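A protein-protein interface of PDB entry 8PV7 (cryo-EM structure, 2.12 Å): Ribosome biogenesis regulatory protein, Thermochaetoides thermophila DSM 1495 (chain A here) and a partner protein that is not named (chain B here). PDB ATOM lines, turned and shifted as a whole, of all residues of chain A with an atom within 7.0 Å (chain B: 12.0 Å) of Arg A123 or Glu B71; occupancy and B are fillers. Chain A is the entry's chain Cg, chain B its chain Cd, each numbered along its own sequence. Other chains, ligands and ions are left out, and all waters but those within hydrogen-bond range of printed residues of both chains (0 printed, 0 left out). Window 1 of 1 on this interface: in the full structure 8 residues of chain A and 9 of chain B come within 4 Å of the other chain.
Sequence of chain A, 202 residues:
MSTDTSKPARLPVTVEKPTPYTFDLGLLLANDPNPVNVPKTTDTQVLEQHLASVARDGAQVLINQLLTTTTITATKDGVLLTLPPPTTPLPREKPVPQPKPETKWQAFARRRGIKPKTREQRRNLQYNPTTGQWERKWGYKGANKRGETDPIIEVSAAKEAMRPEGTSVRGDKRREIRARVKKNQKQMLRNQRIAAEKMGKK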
ATOM      1  N   LYS A 117      30.920  25.830   0.623  1.00  0.00           N
ATOM      2  CA  LYS A 117      29.716  25.698   1.425  1.00  0.00           C
ATOM      3  C   LYS A 117      28.983  27.031   1.499  1.00  0.00           C
ATOM      4  O   LYS A 117      29.587  28.101   1.411  1.00  0.00           O
ATOM      5  CB  LYS A 117      30.070  25.206   2.825  1.00  0.00           C
ATOM      6  CG  LYS A 117      30.474  23.751   2.865  1.00  0.00           C
ATOM      7  CD  LYS A 117      31.518  23.472   3.924  1.00  0.00           C
ATOM      8  CE  LYS A 117      31.101  23.944   5.292  1.00  0.00           C
ATOM      9  NZ  LYS A 117      32.243  23.833   6.229  1.00  0.00           N
ATOM     10  N   THR A 118      27.665  26.959   1.644  1.00  0.00           N
ATOM     11  CA  THR A 118      26.892  28.178   1.803  1.00  0.00           C
ATOM     12  C   THR A 118      27.016  28.699   3.230  1.00  0.00           C
ATOM     13  O   THR A 118      27.404  27.974   4.156  1.00  0.00           O
ATOM     14  CB  THR A 118      25.419  27.955   1.444  1.00  0.00           C
ATOM     15  OG1 THR A 118      24.797  27.099   2.404  1.00  0.00           O
ATOM     16  CG2 THR A 118      25.283  27.336   0.069  1.00  0.00           C
ATOM     17  N   ARG A 119      26.686  29.981   3.395  1.00  0.00           N
ATOM     18  CA  ARG A 119      26.789  30.615   4.702  1.00  0.00           C
ATOM     19  C   ARG A 119      25.792  30.030   5.689  1.00  0.00           C
ATOM     20  O   ARG A 119      26.069  29.984   6.892  1.00  0.00           O
ATOM     21  CB  ARG A 119      26.597  32.123   4.567  1.00  0.00           C
ATOM     22  CG  ARG A 119      27.610  32.779   3.648  1.00  0.00           C
ATOM     23  CD  ARG A 119      27.417  34.278   3.569  1.00  0.00           C
ATOM     24  NE  ARG A 119      27.804  34.942   4.806  1.00  0.00           N
ATOM     25  CZ  ARG A 119      28.995  35.478   5.032  1.00  0.00           C
ATOM     26  NH1 ARG A 119      29.948  35.459   4.118  1.00  0.00           N
ATOM     27  NH2 ARG A 119      29.235  36.047   6.209  1.00  0.00           N
ATOM     28  N   GLU A 120      24.634  29.576   5.208  1.00  0.00           N
ATOM     29  CA  GLU A 120      23.685  28.899   6.085  1.00  0.00           C
ATOM     30  C   GLU A 120      24.186  27.516   6.475  1.00  0.00           C
ATOM     31  O   GLU A 120      23.979  27.069   7.608  1.00  0.00           O
ATOM     32  CB  GLU A 120      22.322  28.806   5.404  1.00  0.00           C
ATOM     33  CG  GLU A 120      21.169  28.467   6.335  1.00  0.00           C
ATOM     34  CD  GLU A 120      21.069  29.391   7.541  1.00  0.00           C
ATOM     35  OE1 GLU A 120      21.270  30.617   7.388  1.00  0.00           O
ATOM     36  OE2 GLU A 120      20.786  28.887   8.648  1.00  0.00           O
ATOM     37  N   GLN A 121      24.844  26.829   5.544  1.00  0.00           N
ATOM     38  CA  GLN A 121      25.391  25.505   5.803  1.00  0.00           C
ATOM     39  C   GLN A 121      26.551  25.545   6.790  1.00  0.00           C
ATOM     40  O   GLN A 121      26.749  24.580   7.534  1.00  0.00           O
ATOM     41  CB  GLN A 121      25.823  24.886   4.472  1.00  0.00           C
ATOM     42  CG  GLN A 121      26.396  23.494   4.508  1.00  0.00           C
ATOM     43  CD  GLN A 121      26.854  23.048   3.133  1.00  0.00           C
ATOM     44  OE1 GLN A 121      26.713  23.781   2.156  1.00  0.00           O
ATOM     45  NE2 GLN A 121      27.404  21.844   3.051  1.00  0.00           N
ATOM     46  N   ARG A 122      27.307  26.640   6.836  1.00  0.00           N
ATOM     47  CA  ARG A 122      28.474  26.715   7.705  1.00  0.00           C
ATOM     48  C   ARG A 122      28.212  27.444   9.027  1.00  0.00           C
ATOM     49  O   ARG A 122      29.168  27.777   9.731  1.00  0.00           O
ATOM     50  CB  ARG A 122      29.638  27.368   6.957  1.00  0.00           C
ATOM     51  CG  ARG A 122      29.473  28.837   6.698  1.00  0.00           C
ATOM     52  CD  ARG A 122      30.335  29.279   5.546  1.00  0.00           C
ATOM     53  NE  ARG A 122      30.530  30.722   5.544  1.00  0.00           N
ATOM     54  CZ  ARG A 122      31.091  31.394   4.551  1.00  0.00           C
ATOM     55  NH1 ARG A 122      31.510  30.785   3.456  1.00  0.00           N
ATOM     56  NH2 ARG A 122      31.232  32.710   4.658  1.00  0.00           N
ATOM     57  N   ARG A 123      26.952  27.678   9.391  1.00  0.00           N
ATOM     58  CA  ARG A 123      26.640  28.360  10.643  1.00  0.00           C
ATOM     59  C   ARG A 123      27.005  27.511  11.858  1.00  0.00           C
ATOM     60  O   ARG A 123      26.916  26.282  11.837  1.00  0.00           O
ATOM     61  CB  ARG A 123      25.157  28.714  10.713  1.00  0.00           C
ATOM     62  CG  ARG A 123      24.766  29.927   9.909  1.00  0.00           C
ATOM     63  CD  ARG A 123      23.385  30.410  10.293  1.00  0.00           C
ATOM     64  NE  ARG A 123      23.305  30.770  11.702  1.00  0.00           N
ATOM     65  CZ  ARG A 123      22.176  31.014  12.350  1.00  0.00           C
ATOM     66  NH1 ARG A 123      21.001  30.907  11.755  1.00  0.00           N
ATOM     67  NH2 ARG A 123      22.227  31.375  13.628  1.00  0.00           N
ATOM     68  N   ASN A 124      27.407  28.188  12.934  1.00  0.00           N
ATOM     69  CA  ASN A 124      27.773  27.531  14.190  1.00  0.00           C
ATOM     70  C   ASN A 124      26.520  27.341  15.045  1.00  0.00           C
ATOM     71  O   ASN A 124      26.360  27.911  16.125  1.00  0.00           O
ATOM     72  CB  ASN A 124      28.829  28.337  14.928  1.00  0.00           C
ATOM     73  CG  ASN A 124      29.416  27.591  16.106  1.00  0.00           C
ATOM     74  OD1 ASN A 124      29.243  26.385  16.240  1.00  0.00           O
ATOM     75  ND2 ASN A 124      30.100  28.312  16.977  1.00  0.00           N
ATOM     76  N   LEU A 125      25.612  26.521  14.531  1.00  0.00           N
ATOM     77  CA  LEU A 125      24.348  26.280  15.204  1.00  0.00           C
ATOM     78  C   LEU A 125      23.787  24.955  14.727  1.00  0.00           C
ATOM     79  O   LEU A 125      23.852  24.638  13.539  1.00  0.00           O
ATOM     80  CB  LEU A 125      23.345  27.406  14.938  1.00  0.00           C
ATOM     81  CG  LEU A 125      22.133  27.431  15.866  1.00  0.00           C
ATOM     82  CD1 LEU A 125      22.580  27.571  17.305  1.00  0.00           C
ATOM     83  CD2 LEU A 125      21.194  28.556  15.492  1.00  0.00           C
ATOM     84  N   GLN A 126      23.240  24.188  15.660  1.00  0.00           N
ATOM     85  CA  GLN A 126      22.556  22.951  15.333  1.00  0.00           C
ATOM     86  C   GLN A 126      21.493  22.714  16.388  1.00  0.00           C
ATOM     87  O   GLN A 126      21.584  23.233  17.502  1.00  0.00           O
ATOM     88  CB  GLN A 126      23.525  21.767  15.256  1.00  0.00           C
ATOM     89  CG  GLN A 126      24.118  21.366  16.589  1.00  0.00           C
ATOM     90  CD  GLN A 126      25.010  20.153  16.485  1.00  0.00           C
ATOM     91  OE1 GLN A 126      25.490  19.814  15.408  1.00  0.00           O
ATOM     92  NE2 GLN A 126      25.227  19.484  17.606  1.00  0.00           N
ATOM     93  N   TRP A 134      18.781  24.555  20.863  1.00  0.00           N
ATOM     94  CA  TRP A 134      19.760  24.951  19.867  1.00  0.00           C
ATOM     95  C   TRP A 134      21.111  25.147  20.538  1.00  0.00           C
ATOM     96  O   TRP A 134      21.204  25.756  21.607  1.00  0.00           O
ATOM     97  CB  TRP A 134      19.327  26.237  19.162  1.00  0.00           C
ATOM     98  CG  TRP A 134      18.139  26.051  18.278  1.00  0.00           C
ATOM     99  CD1 TRP A 134      16.834  26.211  18.624  1.00  0.00           C
ATOM    100  CD2 TRP A 134      18.144  25.667  16.900  1.00  0.00           C
ATOM    101  NE1 TRP A 134      16.025  25.955  17.552  1.00  0.00           N
ATOM    102  CE2 TRP A 134      16.804  25.612  16.481  1.00  0.00           C
ATOM    103  CE3 TRP A 134      19.151  25.359  15.983  1.00  0.00           C
ATOM    104  CZ2 TRP A 134      16.443  25.269  15.184  1.00  0.00           C
ATOM    105  CZ3 TRP A 134      18.792  25.014  14.698  1.00  0.00           C
ATOM    106  CH2 TRP A 134      17.449  24.976  14.309  1.00  0.00           C
ATOM    107  N   LYS A 137      28.027  24.141  17.426  1.00  0.00           N
ATOM    108  CA  LYS A 137      28.816  22.968  17.066  1.00  0.00           C
ATOM    109  C   LYS A 137      30.230  23.028  17.627  1.00  0.00           C
ATOM    110  O   LYS A 137      30.810  21.985  17.940  1.00  0.00           O
ATOM    111  CB  LYS A 137      28.883  22.814  15.548  1.00  0.00           C
ATOM    112  CG  LYS A 137      27.552  22.876  14.841  1.00  0.00           C
ATOM    113  CD  LYS A 137      27.753  22.928  13.341  1.00  0.00           C
ATOM    114  CE  LYS A 137      26.441  22.768  12.607  1.00  0.00           C
ATOM    115  NZ  LYS A 137      26.602  22.951  11.140  1.00  0.00           N
ATOM    116  N   TRP A 138      30.800  24.223  17.737  1.00  0.00           N
ATOM    117  CA  TRP A 138      32.165  24.399  18.205  1.00  0.00           C
ATOM    118  C   TRP A 138      32.230  25.676  19.026  1.00  0.00           C
ATOM    119  O   TRP A 138      31.249  26.410  19.147  1.00  0.00           O
ATOM    120  CB  TRP A 138      33.156  24.434  17.035  1.00  0.00           C
ATOM    121  CG  TRP A 138      32.940  25.573  16.098  1.00  0.00           C
ATOM    122  CD1 TRP A 138      32.081  25.608  15.045  1.00  0.00           C
ATOM    123  CD2 TRP A 138      33.598  26.844  16.119  1.00  0.00           C
ATOM    124  NE1 TRP A 138      32.151  26.820  14.415  1.00  0.00           N
ATOM    125  CE2 TRP A 138      33.079  27.597  15.051  1.00  0.00           C
ATOM    126  CE3 TRP A 138      34.578  27.416  16.934  1.00  0.00           C
ATOM    127  CZ2 TRP A 138      33.503  28.891  14.778  1.00  0.00           C
ATOM    128  CZ3 TRP A 138      34.992  28.699  16.665  1.00  0.00           C
ATOM    129  CH2 TRP A 138      34.457  29.425  15.597  1.00  0.00           C
ATOM    130  N   LYS B  67      13.858  16.624  11.781  1.00  0.00           N
ATOM    131  CA  LYS B  67      13.415  17.577  12.790  1.00  0.00           C
ATOM    132  C   LYS B  67      13.234  18.928  12.111  1.00  0.00           C
ATOM    133  O   LYS B  67      14.205  19.530  11.642  1.00  0.00           O
ATOM    134  CB  LYS B  67      14.424  17.666  13.931  1.00  0.00           C
ATOM    135  CG  LYS B  67      14.365  16.506  14.903  1.00  0.00           C
ATOM    136  CD  LYS B  67      12.976  16.352  15.479  1.00  0.00           C
ATOM    137  CE  LYS B  67      12.920  15.226  16.494  1.00  0.00           C
ATOM    138  NZ  LYS B  67      13.771  15.504  17.678  1.00  0.00           N
ATOM    139  N   ALA B  68      11.996  19.403  12.049  1.00  0.00           N
ATOM    140  CA  ALA B  68      11.678  20.641  11.340  1.00  0.00           C
ATOM    141  C   ALA B  68      11.535  21.756  12.367  1.00  0.00           C
ATOM    142  O   ALA B  68      10.507  21.900  13.023  1.00  0.00           O
ATOM    143  CB  ALA B  68      10.423  20.461  10.500  1.00  0.00           C
ATOM    144  N   VAL B  69      12.584  22.560  12.505  1.00  0.00           N
ATOM    145  CA  VAL B  69      12.690  23.544  13.575  1.00  0.00           C
ATOM    146  C   VAL B  69      13.238  24.848  13.016  1.00  0.00           C
ATOM    147  O   VAL B  69      14.163  24.845  12.200  1.00  0.00           O
ATOM    148  CB  VAL B  69      13.583  23.031  14.724  1.00  0.00           C
ATOM    149  CG1 VAL B  69      12.786  22.149  15.652  1.00  0.00           C
ATOM    150  CG2 VAL B  69      14.764  22.269  14.165  1.00  0.00           C
ATOM    151  N   ILE B  70      12.667  25.962  13.459  1.00  0.00           N
ATOM    152  CA  ILE B  70      13.120  27.293  13.076  1.00  0.00           C
ATOM    153  C   ILE B  70      13.820  27.899  14.281  1.00  0.00           C
ATOM    154  O   ILE B  70      13.211  28.054  15.346  1.00  0.00           O
ATOM    155  CB  ILE B  70      11.955  28.185  12.619  1.00  0.00           C
ATOM    156  CG1 ILE B  70      11.177  27.534  11.474  1.00  0.00           C
ATOM    157  CG2 ILE B  70      12.471  29.550  12.200  1.00  0.00           C
ATOM    158  CD1 ILE B  70      11.881  27.573  10.151  1.00  0.00           C
ATOM    159  N   GLU B  71      15.085  28.246  14.119  1.00  0.00           N
ATOM    160  CA  GLU B  71      15.817  28.815  15.235  1.00  0.00           C
ATOM    161  C   GLU B  71      15.395  30.263  15.477  1.00  0.00           C
ATOM    162  O   GLU B  71      14.951  30.952  14.555  1.00  0.00           O
ATOM    163  CB  GLU B  71      17.326  28.732  14.986  1.00  0.00           C
ATOM    164  CG  GLU B  71      17.947  29.890  14.222  1.00  0.00           C
ATOM    165  CD  GLU B  71      17.757  29.787  12.723  1.00  0.00           C
ATOM    166  OE1 GLU B  71      17.179  28.786  12.252  1.00  0.00           O
ATOM    167  OE2 GLU B  71      18.191  30.713  12.010  1.00  0.00           O
ATOM    168  N   PRO B  72      15.468  30.727  16.721  1.00  0.00           N
ATOM    169  CA  PRO B  72      15.278  32.157  16.974  1.00  0.00           C
ATOM    170  C   PRO B  72      16.417  32.963  16.376  1.00  0.00           C
ATOM    171  O   PRO B  72      17.588  32.591  16.473  1.00  0.00           O
ATOM    172  CB  PRO B  72      15.249  32.251  18.503  1.00  0.00           C
ATOM    173  CG  PRO B  72      15.892  31.008  18.976  1.00  0.00           C
ATOM    174  CD  PRO B  72      15.581  29.958  17.968  1.00  0.00           C
ATOM    175  N   ASN B  73      16.057  34.065  15.732  1.00  0.00           N
ATOM    176  CA  ASN B  73      17.000  34.864  14.968  1.00  0.00           C
ATOM    177  C   ASN B  73      16.435  36.266  14.840  1.00  0.00           C
ATOM    178  O   ASN B  73      15.246  36.434  14.574  1.00  0.00           O
ATOM    179  CB  ASN B  73      17.239  34.248  13.584  1.00  0.00           C
ATOM    180  CG  ASN B  73      18.515  34.725  12.935  1.00  0.00           C
ATOM    181  OD1 ASN B  73      18.876  35.894  13.018  1.00  0.00           O
ATOM    182  ND2 ASN B  73      19.205  33.815  12.269  1.00  0.00           N
ATOM    183  N   ARG B  74      17.302  37.265  15.015  1.00  0.00           N
ATOM    184  CA  ARG B  74      16.861  38.650  14.906  1.00  0.00           C
ATOM    185  C   ARG B  74      16.543  39.033  13.466  1.00  0.00           C
ATOM    186  O   ARG B  74      15.823  40.007  13.234  1.00  0.00           O
ATOM    187  CB  ARG B  74      17.924  39.587  15.474  1.00  0.00           C
ATOM    188  N   LYS B  75      17.055  38.273  12.493  1.00  0.00           N
ATOM    189  CA  LYS B  75      16.823  38.601  11.090  1.00  0.00           C
ATOM    190  C   LYS B  75      15.366  38.405  10.686  1.00  0.00           C
ATOM    191  O   LYS B  75      14.915  38.999   9.703  1.00  0.00           O
ATOM    192  CB  LYS B  75      17.738  37.763  10.192  1.00  0.00           C
ATOM    193  CG  LYS B  75      17.295  36.322  10.034  1.00  0.00           C
ATOM    194  CD  LYS B  75      17.797  35.688   8.756  1.00  0.00           C
ATOM    195  CE  LYS B  75      19.278  35.433   8.799  1.00  0.00           C
ATOM    196  NZ  LYS B  75      19.711  34.628   7.634  1.00  0.00           N
ATOM    197  N   TRP B  76      14.608  37.601  11.440  1.00  0.00           N
ATOM    198  CA  TRP B  76      13.216  37.348  11.094  1.00  0.00           C
ATOM    199  C   TRP B  76      12.331  38.564  11.305  1.00  0.00           C
ATOM    200  O   TRP B  76      11.226  38.609  10.759  1.00  0.00           O
ATOM    201  CB  TRP B  76      12.630  36.194  11.912  1.00  0.00           C
ATOM    202  CG  TRP B  76      13.372  34.886  11.936  1.00  0.00           C
ATOM    203  CD1 TRP B  76      13.621  34.133  13.038  1.00  0.00           C
ATOM    204  CD2 TRP B  76      13.920  34.159  10.824  1.00  0.00           C
ATOM    205  NE1 TRP B  76      14.291  32.996  12.697  1.00  0.00           N
ATOM    206  CE2 TRP B  76      14.494  32.987  11.344  1.00  0.00           C
ATOM    207  CE3 TRP B  76      13.987  34.387   9.446  1.00  0.00           C
ATOM    208  CZ2 TRP B  76      15.126  32.049  10.541  1.00  0.00           C
ATOM    209  CZ3 TRP B  76      14.617  33.457   8.653  1.00  0.00           C
ATOM    210  CH2 TRP B  76      15.178  32.301   9.200  1.00  0.00           C
ATOM    211  N   PHE B  77      12.785  39.544  12.081  1.00  0.00           N
ATOM    212  CA  PHE B  77      11.951  40.659  12.500  1.00  0.00           C
ATOM    213  C   PHE B  77      12.433  41.990  11.937  1.00  0.00           C
ATOM    214  O   PHE B  77      11.972  43.045  12.376  1.00  0.00           O
ATOM    215  CB  PHE B  77      11.884  40.705  14.026  1.00  0.00           C
ATOM    216  CG  PHE B  77      11.262  39.483  14.633  1.00  0.00           C
ATOM    217  CD1 PHE B  77      12.037  38.386  14.976  1.00  0.00           C
ATOM    218  CD2 PHE B  77       9.898  39.422  14.841  1.00  0.00           C
ATOM    219  CE1 PHE B  77      11.459  37.261  15.515  1.00  0.00           C
ATOM    220  CE2 PHE B  77       9.319  38.298  15.389  1.00  0.00           C
ATOM    221  CZ  PHE B  77      10.103  37.216  15.725  1.00  0.00           C
ATOM    222  N   THR B  78      13.348  41.962  10.980  1.00  0.00           N
ATOM    223  CA  THR B  78      13.846  43.165  10.332  1.00  0.00           C
ATOM    224  C   THR B  78      13.244  43.296   8.940  1.00  0.00           C
ATOM    225  O   THR B  78      12.588  42.388   8.427  1.00  0.00           O
ATOM    226  CB  THR B  78      15.377  43.153  10.248  1.00  0.00           C
ATOM    227  OG1 THR B  78      15.803  42.154   9.315  1.00  0.00           O
ATOM    228  CG2 THR B  78      15.984  42.857  11.600  1.00  0.00           C
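The side-chain carboxylate (OE2) of Glu B71 lies within salt-bridge range of the guanidinium group (NH1) of Arg A123.
The side-chain amide nitrogen (ND2) of Asn B73 sits close to the guanidinium group (NH1) of Arg A123 (3.5 Å).
OE2 of Glu B71 is in hydrogen-bond range of ND2 of Asn B73 (3.3 Å).
The backbone carbonyl oxygen (O) of Glu B71 lies within hydrogen-bond range of the indole nitrogen (NE1) of Trp B76 (2.8 Å).
OD1 of Asn B73 is in hydrogen-bond range of N of Lys B75 (3.0 Å).
The guanidinium group (NH1) of Arg A123 is in salt-bridge range of the side-chain carboxylate (OE2) of Glu A120 (3.7 Å).
The backbone carbonyl oxygen (O) of Arg A123 sits at hydrogen-bond distance from the side-chain amino group (NZ) of Lys A137.
Leu A125 touches Glu B71.
Trp A134 touches Val B69 (CZ2 to CG2, 3.6 Å).
Ile B70 touches Trp A134 (C to CZ2, 3.8 Å).
Glu B71 touches Trp A134.
Arg A119 touches none of the printed residues of chain B.
No residue of chain B comes within 4 Å of Glu A120.
Printed residues of chain B within 4 Å of Arg A123: Glu B71 (2.8 Å) and Asn B73 (3.5 Å).
No residue of chain B comes within 4 Å of Asn A124.
Gln A126 touches none of the printed residues of chain B.
Of the printed residues of chain B, Trp A134 touches Val B69, Ile B70 and Glu B71.
Printed residues of chain A within 4 Å of Val B69: Trp A134 (3.6 Å).
Glu B71 touches just these residues of chain A: Arg A123, Leu A125 and Trp A134.
Of the printed residues of chain A, Asn B73 touches Arg A123 (3.5 Å).
The nearest residue of chain B that does not touch Arg A123 is Pro B72 (5.6 Å).
The nearest residue of chain A that does not touch Glu B71 is Glu A120 (4.6 Å).
Of the 13 printed residues of chain A, 3 touch a printed residue of chain B.
Among the printed residues, 6 pairs touch across the chains.
Among the printed residues, Asp or Glu carboxylates within 4 Å of a Lys or Arg side-chain nitrogen of the other chain: Arg A123 with Glu B71.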
